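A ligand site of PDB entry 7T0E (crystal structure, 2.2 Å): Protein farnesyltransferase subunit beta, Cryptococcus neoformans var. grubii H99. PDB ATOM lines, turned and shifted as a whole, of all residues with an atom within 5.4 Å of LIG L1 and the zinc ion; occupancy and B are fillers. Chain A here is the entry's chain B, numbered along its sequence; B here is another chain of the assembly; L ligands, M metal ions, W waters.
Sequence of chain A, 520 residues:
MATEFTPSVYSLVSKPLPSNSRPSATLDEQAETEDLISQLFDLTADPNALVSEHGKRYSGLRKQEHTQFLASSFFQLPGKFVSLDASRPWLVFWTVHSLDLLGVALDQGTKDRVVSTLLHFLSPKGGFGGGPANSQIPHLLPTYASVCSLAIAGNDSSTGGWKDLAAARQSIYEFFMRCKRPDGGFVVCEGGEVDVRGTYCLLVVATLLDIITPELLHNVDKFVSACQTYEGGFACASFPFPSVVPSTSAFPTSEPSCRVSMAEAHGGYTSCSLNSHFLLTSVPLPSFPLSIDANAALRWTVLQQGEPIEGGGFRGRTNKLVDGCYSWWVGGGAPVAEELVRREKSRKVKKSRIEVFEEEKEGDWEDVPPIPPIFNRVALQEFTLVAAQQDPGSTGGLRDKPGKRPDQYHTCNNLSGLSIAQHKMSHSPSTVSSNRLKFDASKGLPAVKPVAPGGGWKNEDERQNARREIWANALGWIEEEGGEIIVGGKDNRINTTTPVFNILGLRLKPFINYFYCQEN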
ATOM      1  N   LEU A  84      -8.641 -26.634  -6.371  1.00  0.00           N
ATOM      2  CA  LEU A  84      -7.823 -27.612  -7.077  1.00  0.00           C
ATOM      3  C   LEU A  84      -7.890 -28.990  -6.445  1.00  0.00           C
ATOM      4  O   LEU A  84      -7.077 -29.862  -6.776  1.00  0.00           O
ATOM      5  CB  LEU A  84      -6.369 -27.129  -7.135  1.00  0.00           C
ATOM      6  CG  LEU A  84      -6.116 -25.899  -8.004  1.00  0.00           C
ATOM      7  CD1 LEU A  84      -4.774 -25.274  -7.691  1.00  0.00           C
ATOM      8  CD2 LEU A  84      -6.207 -26.269  -9.468  1.00  0.00           C
ATOM      9  N   SER A  87      -7.736 -31.712  -8.795  1.00  0.00           N
ATOM     10  CA  SER A  87      -6.637 -31.626  -9.740  1.00  0.00           C
ATOM     11  C   SER A  87      -5.296 -31.827  -9.058  1.00  0.00           C
ATOM     12  O   SER A  87      -4.269 -31.306  -9.519  1.00  0.00           O
ATOM     13  CB  SER A  87      -6.665 -30.288 -10.481  1.00  0.00           C
ATOM     14  OG  SER A  87      -7.796 -30.188 -11.329  1.00  0.00           O
ATOM     15  N   TRP A  90      -2.269 -32.834 -10.977  1.00  0.00           N
ATOM     16  CA  TRP A  90      -1.683 -31.725 -11.709  1.00  0.00           C
ATOM     17  C   TRP A  90      -0.744 -30.905 -10.822  1.00  0.00           C
ATOM     18  O   TRP A  90       0.297 -30.436 -11.291  1.00  0.00           O
ATOM     19  CB  TRP A  90      -2.770 -30.845 -12.302  1.00  0.00           C
ATOM     20  CG  TRP A  90      -3.438 -31.473 -13.474  1.00  0.00           C
ATOM     21  CD1 TRP A  90      -4.653 -32.083 -13.496  1.00  0.00           C
ATOM     22  CD2 TRP A  90      -2.908 -31.580 -14.794  1.00  0.00           C
ATOM     23  NE1 TRP A  90      -4.928 -32.555 -14.755  1.00  0.00           N
ATOM     24  CE2 TRP A  90      -3.870 -32.268 -15.574  1.00  0.00           C
ATOM     25  CE3 TRP A  90      -1.719 -31.170 -15.408  1.00  0.00           C
ATOM     26  CZ2 TRP A  90      -3.675 -32.538 -16.920  1.00  0.00           C
ATOM     27  CZ3 TRP A  90      -1.527 -31.446 -16.747  1.00  0.00           C
ATOM     28  CH2 TRP A  90      -2.503 -32.122 -17.496  1.00  0.00           C
ATOM     29  N   TRP A  94       2.972 -30.402 -12.142  1.00  0.00           N
ATOM     30  CA  TRP A  94       3.538 -29.057 -12.256  1.00  0.00           C
ATOM     31  C   TRP A  94       4.763 -28.892 -11.376  1.00  0.00           C
ATOM     32  O   TRP A  94       5.695 -28.165 -11.741  1.00  0.00           O
ATOM     33  CB  TRP A  94       2.479 -28.013 -11.879  1.00  0.00           C
ATOM     34  CG  TRP A  94       1.314 -27.954 -12.827  1.00  0.00           C
ATOM     35  CD1 TRP A  94       1.322 -28.233 -14.165  1.00  0.00           C
ATOM     36  CD2 TRP A  94      -0.041 -27.608 -12.492  1.00  0.00           C
ATOM     37  NE1 TRP A  94       0.063 -28.069 -14.682  1.00  0.00           N
ATOM     38  CE2 TRP A  94      -0.788 -27.690 -13.684  1.00  0.00           C
ATOM     39  CE3 TRP A  94      -0.683 -27.237 -11.320  1.00  0.00           C
ATOM     40  CZ2 TRP A  94      -2.160 -27.419 -13.723  1.00  0.00           C
ATOM     41  CZ3 TRP A  94      -2.046 -26.966 -11.355  1.00  0.00           C
ATOM     42  CH2 TRP A  94      -2.761 -27.050 -12.548  1.00  0.00           C
ATOM     43  N   LEU A 141      -7.745 -36.538 -17.539  1.00  0.00           N
ATOM     44  CA  LEU A 141      -6.720 -35.512 -17.350  1.00  0.00           C
ATOM     45  C   LEU A 141      -5.817 -35.826 -16.164  1.00  0.00           C
ATOM     46  O   LEU A 141      -4.590 -35.749 -16.301  1.00  0.00           O
ATOM     47  CB  LEU A 141      -7.364 -34.128 -17.217  1.00  0.00           C
ATOM     48  CG  LEU A 141      -7.542 -33.320 -18.503  1.00  0.00           C
ATOM     49  CD1 LEU A 141      -8.418 -34.063 -19.517  1.00  0.00           C
ATOM     50  CD2 LEU A 141      -8.123 -31.952 -18.209  1.00  0.00           C
ATOM     51  N   ARG A 197      -8.532 -32.043 -25.188  1.00  0.00           N
ATOM     52  CA  ARG A 197      -7.701 -32.298 -24.012  1.00  0.00           C
ATOM     53  C   ARG A 197      -7.762 -33.769 -23.626  1.00  0.00           C
ATOM     54  O   ARG A 197      -6.733 -34.375 -23.284  1.00  0.00           O
ATOM     55  CB  ARG A 197      -8.133 -31.444 -22.828  1.00  0.00           C
ATOM     56  CG  ARG A 197      -8.064 -29.941 -22.999  1.00  0.00           C
ATOM     57  CD  ARG A 197      -8.774 -29.307 -21.822  1.00  0.00           C
ATOM     58  NE  ARG A 197     -10.077 -29.941 -21.605  1.00  0.00           N
ATOM     59  CZ  ARG A 197     -10.750 -29.952 -20.464  1.00  0.00           C
ATOM     60  NH1 ARG A 197     -10.236 -29.365 -19.389  1.00  0.00           N
ATOM     61  NH2 ARG A 197     -11.919 -30.565 -20.389  1.00  0.00           N
ATOM     62  N   ASP A 323       0.176 -14.280 -22.604  1.00  0.00           N
ATOM     63  CA  ASP A 323       0.158 -14.993 -21.339  1.00  0.00           C
ATOM     64  C   ASP A 323       1.327 -15.965 -21.332  1.00  0.00           C
ATOM     65  O   ASP A 323       1.515 -16.715 -22.295  1.00  0.00           O
ATOM     66  CB  ASP A 323      -1.178 -15.729 -21.149  1.00  0.00           C
ATOM     67  CG  ASP A 323      -1.303 -16.446 -19.810  1.00  0.00           C
ATOM     68  OD1 ASP A 323      -0.285 -16.920 -19.263  1.00  0.00           O
ATOM     69  OD2 ASP A 323      -2.436 -16.546 -19.304  1.00  0.00           O
ATOM     70  N   GLY A 324       2.084 -15.963 -20.239  1.00  0.00           N
ATOM     71  CA  GLY A 324       3.284 -16.792 -20.175  1.00  0.00           C
ATOM     72  C   GLY A 324       3.025 -18.264 -20.353  1.00  0.00           C
ATOM     73  O   GLY A 324       3.878 -18.990 -20.886  1.00  0.00           O
ATOM     74  N   CYS A 325       1.858 -18.745 -19.919  1.00  0.00           N
ATOM     75  CA  CYS A 325       1.573 -20.178 -20.037  1.00  0.00           C
ATOM     76  C   CYS A 325       1.486 -20.631 -21.485  1.00  0.00           C
ATOM     77  O   CYS A 325       1.714 -21.812 -21.766  1.00  0.00           O
ATOM     78  CB  CYS A 325       0.294 -20.532 -19.284  1.00  0.00           C
ATOM     79  SG  CYS A 325      -1.250 -20.005 -20.076  1.00  0.00           S
ATOM     80  N   TYR A 326       1.168 -19.719 -22.414  1.00  0.00           N
ATOM     81  CA  TYR A 326       1.107 -20.083 -23.820  1.00  0.00           C
ATOM     82  C   TYR A 326       2.475 -20.177 -24.473  1.00  0.00           C
ATOM     83  O   TYR A 326       2.564 -20.503 -25.668  1.00  0.00           O
ATOM     84  CB  TYR A 326       0.236 -19.085 -24.592  1.00  0.00           C
ATOM     85  CG  TYR A 326      -1.192 -19.055 -24.107  1.00  0.00           C
ATOM     86  CD1 TYR A 326      -1.957 -20.209 -24.087  1.00  0.00           C
ATOM     87  CD2 TYR A 326      -1.770 -17.873 -23.663  1.00  0.00           C
ATOM     88  CE1 TYR A 326      -3.262 -20.185 -23.636  1.00  0.00           C
ATOM     89  CE2 TYR A 326      -3.072 -17.842 -23.219  1.00  0.00           C
ATOM     90  CZ  TYR A 326      -3.814 -18.998 -23.204  1.00  0.00           C
ATOM     91  OH  TYR A 326      -5.119 -18.974 -22.753  1.00  0.00           O
ATOM     92  N   ASP A 400       1.329 -15.492 -15.171  1.00  0.00           N
ATOM     93  CA  ASP A 400       0.701 -15.128 -16.445  1.00  0.00           C
ATOM     94  C   ASP A 400       1.250 -13.805 -16.958  1.00  0.00           C
ATOM     95  O   ASP A 400       1.785 -13.733 -18.082  1.00  0.00           O
ATOM     96  CB  ASP A 400      -0.820 -15.082 -16.228  1.00  0.00           C
ATOM     97  CG  ASP A 400      -1.565 -14.248 -17.275  1.00  0.00           C
ATOM     98  OD1 ASP A 400      -1.042 -13.963 -18.371  1.00  0.00           O
ATOM     99  OD2 ASP A 400      -2.727 -13.877 -16.988  1.00  0.00           O
ATOM    100  N   ASP A 407       1.684 -18.988  -9.888  1.00  0.00           N
ATOM    101  CA  ASP A 407       1.091 -20.247  -9.450  1.00  0.00           C
ATOM    102  C   ASP A 407       1.871 -21.400 -10.041  1.00  0.00           C
ATOM    103  O   ASP A 407       2.757 -21.214 -10.890  1.00  0.00           O
ATOM    104  CB  ASP A 407      -0.402 -20.334  -9.819  1.00  0.00           C
ATOM    105  CG  ASP A 407      -0.653 -20.101 -11.293  1.00  0.00           C
ATOM    106  OD1 ASP A 407      -0.173 -20.892 -12.126  1.00  0.00           O
ATOM    107  OD2 ASP A 407      -1.356 -19.111 -11.612  1.00  0.00           O
ATOM    108  N   GLN A 408       1.545 -22.617  -9.593  1.00  0.00           N
ATOM    109  CA  GLN A 408       2.262 -23.796 -10.057  1.00  0.00           C
ATOM    110  C   GLN A 408       2.011 -24.058 -11.530  1.00  0.00           C
ATOM    111  O   GLN A 408       2.926 -24.526 -12.238  1.00  0.00           O
ATOM    112  CB  GLN A 408       1.857 -25.014  -9.215  1.00  0.00           C
ATOM    113  CG  GLN A 408       2.522 -25.059  -7.850  1.00  0.00           C
ATOM    114  CD  GLN A 408       1.545 -25.327  -6.729  1.00  0.00           C
ATOM    115  OE1 GLN A 408       0.768 -24.450  -6.353  1.00  0.00           O
ATOM    116  NE2 GLN A 408       1.582 -26.538  -6.192  1.00  0.00           N
ATOM    117  N   TYR A 409       0.807 -23.772 -12.022  1.00  0.00           N
ATOM    118  CA  TYR A 409       0.485 -24.012 -13.427  1.00  0.00           C
ATOM    119  C   TYR A 409       1.310 -23.109 -14.341  1.00  0.00           C
ATOM    120  O   TYR A 409       1.896 -23.585 -15.325  1.00  0.00           O
ATOM    121  CB  TYR A 409      -1.011 -23.806 -13.662  1.00  0.00           C
ATOM    122  CG  TYR A 409      -1.381 -23.598 -15.111  1.00  0.00           C
ATOM    123  CD1 TYR A 409      -1.553 -24.682 -15.964  1.00  0.00           C
ATOM    124  CD2 TYR A 409      -1.579 -22.323 -15.626  1.00  0.00           C
ATOM    125  CE1 TYR A 409      -1.898 -24.500 -17.290  1.00  0.00           C
ATOM    126  CE2 TYR A 409      -1.924 -22.128 -16.953  1.00  0.00           C
ATOM    127  CZ  TYR A 409      -2.086 -23.215 -17.779  1.00  0.00           C
ATOM    128  OH  TYR A 409      -2.423 -23.033 -19.100  1.00  0.00           O
ATOM    129  N   HIS A 410       1.359 -21.808 -14.050  1.00  0.00           N
ATOM    130  CA  HIS A 410       2.152 -20.906 -14.885  1.00  0.00           C
ATOM    131  C   HIS A 410       3.643 -21.111 -14.691  1.00  0.00           C
ATOM    132  O   HIS A 410       4.422 -20.806 -15.598  1.00  0.00           O
ATOM    133  CB  HIS A 410       1.766 -19.457 -14.593  1.00  0.00           C
ATOM    134  CG  HIS A 410       0.428 -19.069 -15.127  1.00  0.00           C
ATOM    135  ND1 HIS A 410      -0.732 -19.144 -14.373  1.00  0.00           N
ATOM    136  CD2 HIS A 410       0.046 -18.603 -16.339  1.00  0.00           C
ATOM    137  CE1 HIS A 410      -1.753 -18.739 -15.096  1.00  0.00           C
ATOM    138  NE2 HIS A 410      -1.316 -18.408 -16.299  1.00  0.00           N
ATOM    139  N   TYR B 123     -15.571 -25.862 -15.928  1.00  0.00           N
ATOM    140  CA  TYR B 123     -15.950 -26.824 -16.959  1.00  0.00           C
ATOM    141  C   TYR B 123     -17.161 -27.638 -16.524  1.00  0.00           C
ATOM    142  O   TYR B 123     -18.011 -27.987 -17.340  1.00  0.00           O
ATOM    143  CB  TYR B 123     -14.788 -27.775 -17.247  1.00  0.00           C
ATOM    144  CG  TYR B 123     -13.724 -27.270 -18.186  1.00  0.00           C
ATOM    145  CD1 TYR B 123     -13.871 -27.388 -19.570  1.00  0.00           C
ATOM    146  CD2 TYR B 123     -12.552 -26.710 -17.700  1.00  0.00           C
ATOM    147  CE1 TYR B 123     -12.884 -26.946 -20.429  1.00  0.00           C
ATOM    148  CE2 TYR B 123     -11.567 -26.259 -18.554  1.00  0.00           C
ATOM    149  CZ  TYR B 123     -11.734 -26.387 -19.914  1.00  0.00           C
ATOM    150  OH  TYR B 123     -10.749 -25.936 -20.768  1.00  0.00           O
HETATM  151  C1  LIG L   1      -6.830 -27.936 -13.414  1.00  0.00           C
HETATM  152  C2  LIG L   1      -7.756 -23.772 -14.923  1.00  0.00           C
HETATM  153  C3  LIG L   1      -7.744 -22.197 -15.115  1.00  0.00           C
HETATM  154  C4  LIG L   1      -5.650 -19.964 -16.918  1.00  0.00           C
HETATM  155  C5  LIG L   1      -4.393 -19.379 -16.711  1.00  0.00           C
HETATM  156  C6  LIG L   1      -7.096 -22.197 -18.842  1.00  0.00           C
HETATM  157  C7  LIG L   1      -8.476 -24.178 -18.616  1.00  0.00           C
HETATM  158  C8  LIG L   1      -3.270 -22.860 -10.440  1.00  0.00           C
HETATM  159  C9  LIG L   1      -4.386 -22.009 -11.094  1.00  0.00           C
HETATM  160  C10 LIG L   1      -4.212 -21.903 -12.624  1.00  0.00           C
HETATM  161  C11 LIG L   1      -5.582 -21.663 -13.394  1.00  0.00           C
HETATM  162  C12 LIG L   1      -5.472 -22.102 -14.949  1.00  0.00           C
HETATM  163  C13 LIG L   1      -5.246 -23.590 -14.991  1.00  0.00           C
HETATM  164  C14 LIG L   1      -6.323 -25.925 -14.662  1.00  0.00           C
HETATM  165  C15 LIG L   1      -6.935 -26.544 -13.584  1.00  0.00           C
HETATM  166  C16 LIG L   1      -6.111 -28.681 -14.326  1.00  0.00           C
HETATM  167  C17 LIG L   1      -5.486 -28.056 -15.408  1.00  0.00           C
HETATM  168  C18 LIG L   1      -5.601 -26.678 -15.580  1.00  0.00           C
HETATM  169  C19 LIG L   1      -6.655 -20.421 -15.783  1.00  0.00           C
HETATM  170  C20 LIG L   1      -4.727 -19.579 -18.866  1.00  0.00           C
HETATM  171  C21 LIG L   1      -7.010 -20.639 -18.976  1.00  0.00           C
HETATM  172  C22 LIG L   1      -8.362 -22.792 -18.740  1.00  0.00           C
HETATM  173  C23 LIG L   1      -7.347 -24.970 -18.619  1.00  0.00           C
HETATM  174  C24 LIG L   1      -6.080 -24.374 -18.721  1.00  0.00           C
HETATM  175  C25 LIG L   1      -5.959 -22.981 -18.835  1.00  0.00           C
HETATM  176  N1  LIG L   1      -6.440 -24.436 -14.854  1.00  0.00           N
HETATM  177  N2  LIG L   1      -6.603 -21.718 -15.668  1.00  0.00           N
HETATM  178  N3  LIG L   1      -3.861 -19.156 -17.932  1.00  0.00           N
HETATM  179  N4  LIG L   1      -5.804 -20.075 -18.259  1.00  0.00           N
HETATM  180  O1  LIG L   1      -8.773 -24.383 -14.823  1.00  0.00           O
HETATM  181 BR1  LIG L   1      -7.531 -26.897 -18.454  1.00  0.00          BR
HETATM  182 CL1  LIG L   1      -4.557 -29.019 -16.590  1.00  0.00          CL
HETATM  183  C1  LG2 L   2      -9.396 -19.873 -22.112  1.00  0.00           C
HETATM  184  O1  LG2 L   2      -9.577 -19.295 -20.852  1.00  0.00           O
HETATM  185  C2  LG2 L   2     -10.409 -20.993 -22.302  1.00  0.00           C
HETATM  186  C3  LG2 L   2     -10.019 -22.248 -22.347  1.00  0.00           C
HETATM  187  C4  LG2 L   2     -11.079 -23.336 -22.531  1.00  0.00           C
HETATM  188  C5  LG2 L   2      -8.539 -22.582 -22.205  1.00  0.00           C
HETATM  189  C6  LG2 L   2      -8.147 -24.020 -22.567  1.00  0.00           C
HETATM  190  C7  LG2 L   2      -6.640 -24.012 -22.333  1.00  0.00           C
HETATM  191  C8  LG2 L   2      -5.793 -25.026 -22.307  1.00  0.00           C
HETATM  192  C9  LG2 L   2      -4.346 -24.665 -22.036  1.00  0.00           C
HETATM  193  C10 LG2 L   2      -6.156 -26.490 -22.522  1.00  0.00           C
HETATM  194  C11 LG2 L   2      -5.404 -27.316 -21.465  1.00  0.00           C
HETATM  195  C12 LG2 L   2      -4.689 -28.536 -22.056  1.00  0.00           C
HETATM  196  C13 LG2 L   2      -4.531 -29.617 -21.312  1.00  0.00           C
HETATM  197  C14 LG2 L   2      -3.822 -30.852 -21.864  1.00  0.00           C
HETATM  198  C15 LG2 L   2      -5.055 -29.658 -19.879  1.00  0.00           C
HETATM  199  P1  LG2 L   2      -9.179 -17.705 -20.644  1.00  0.00           P
HETATM  200  O2  LG2 L   2     -10.188 -16.850 -21.371  1.00  0.00           O
HETATM  201  O3  LG2 L   2      -9.180 -17.370 -19.166  1.00  0.00           O
HETATM  202  O4  LG2 L   2      -7.681 -17.446 -21.273  1.00  0.00           O
HETATM  203  P2  LG2 L   2      -7.402 -16.578 -22.643  1.00  0.00           P
HETATM  204  O5  LG2 L   2      -8.061 -15.238 -22.524  1.00  0.00           O
HETATM  205  O6  LG2 L   2      -7.949 -17.325 -23.845  1.00  0.00           O
HETATM  206  O7  LG2 L   2      -5.908 -16.387 -22.820  1.00  0.00           O
HETATM  207 ZN    ZN M   1      -1.991 -18.529 -18.493  1.00  0.00          ZN
HETATM  208  O   HOH W   1      -9.785 -27.073 -14.879  1.00  0.00           O
HETATM  209  O   HOH W   2      -4.215 -18.645 -13.255  1.00  0.00           O
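The side-chain hydroxyl (OH) of Tyr 326 lies within hydrogen-bond range of an oxygen (O7) of LG2 L2 (2.7 Å).
SG of Cys 325 sits close to OH of Tyr 409, at 3.4 Å. N of Tyr 409 is in hydrogen-bond range of OD1 of Asp 407, 3.0 Å away. The side-chain carboxylate (OD1) of Asp 407 is in hydrogen-bond range of the backbone NH (N) of His 410, at 2.6 Å.
CD1 of Leu 84 touches C8 of LIG L1, 3.96 Å away. Ser 87 touches LIG L1. Trp 90 touches LIG L1 (CE2 to CL1, 3.5 Å). Trp 94 touches LIG L1 (CZ2 to C17, 3.8 Å). NH1 of Arg 197 touches BR1 of LIG L1 (3.8 Å). Tyr 326 touches LIG L1. Asp 407 touches LIG L1. OH of Tyr 409 touches C25 of LIG L1, at 3.5 Å. Tyr 123 of chain B touches LIG L1. Hydrophobic or aromatic side chains within 4 Å of LIG L1: Leu 84, Trp 90, Trp 94, Tyr 409, His 410 and Tyr 123 of chain B.
Tyr 409 touches the zinc ion (CE2 to ZN, 3.9 Å). Four residues have an atom within 4 Å of the zinc ion: Asp 323, Cys 325, Tyr 409 and His 410. Along chain A the residues within 4 Å of the zinc ion span positions 323 to 410. The nearest printed residue that does not touch the zinc ion is Asp 400 (4.3 Å).
The zinc ion is bound by N3 of LIG L1 (2.1 Å), OD2 of Asp 323 (2.2 Å), SG of Cys 325 (2.3 Å), NE2 of His 410 (2.3 Å) and OD1 of Asp 323 (2.5 Å). The zinc ion has five donor atoms within binding distance.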
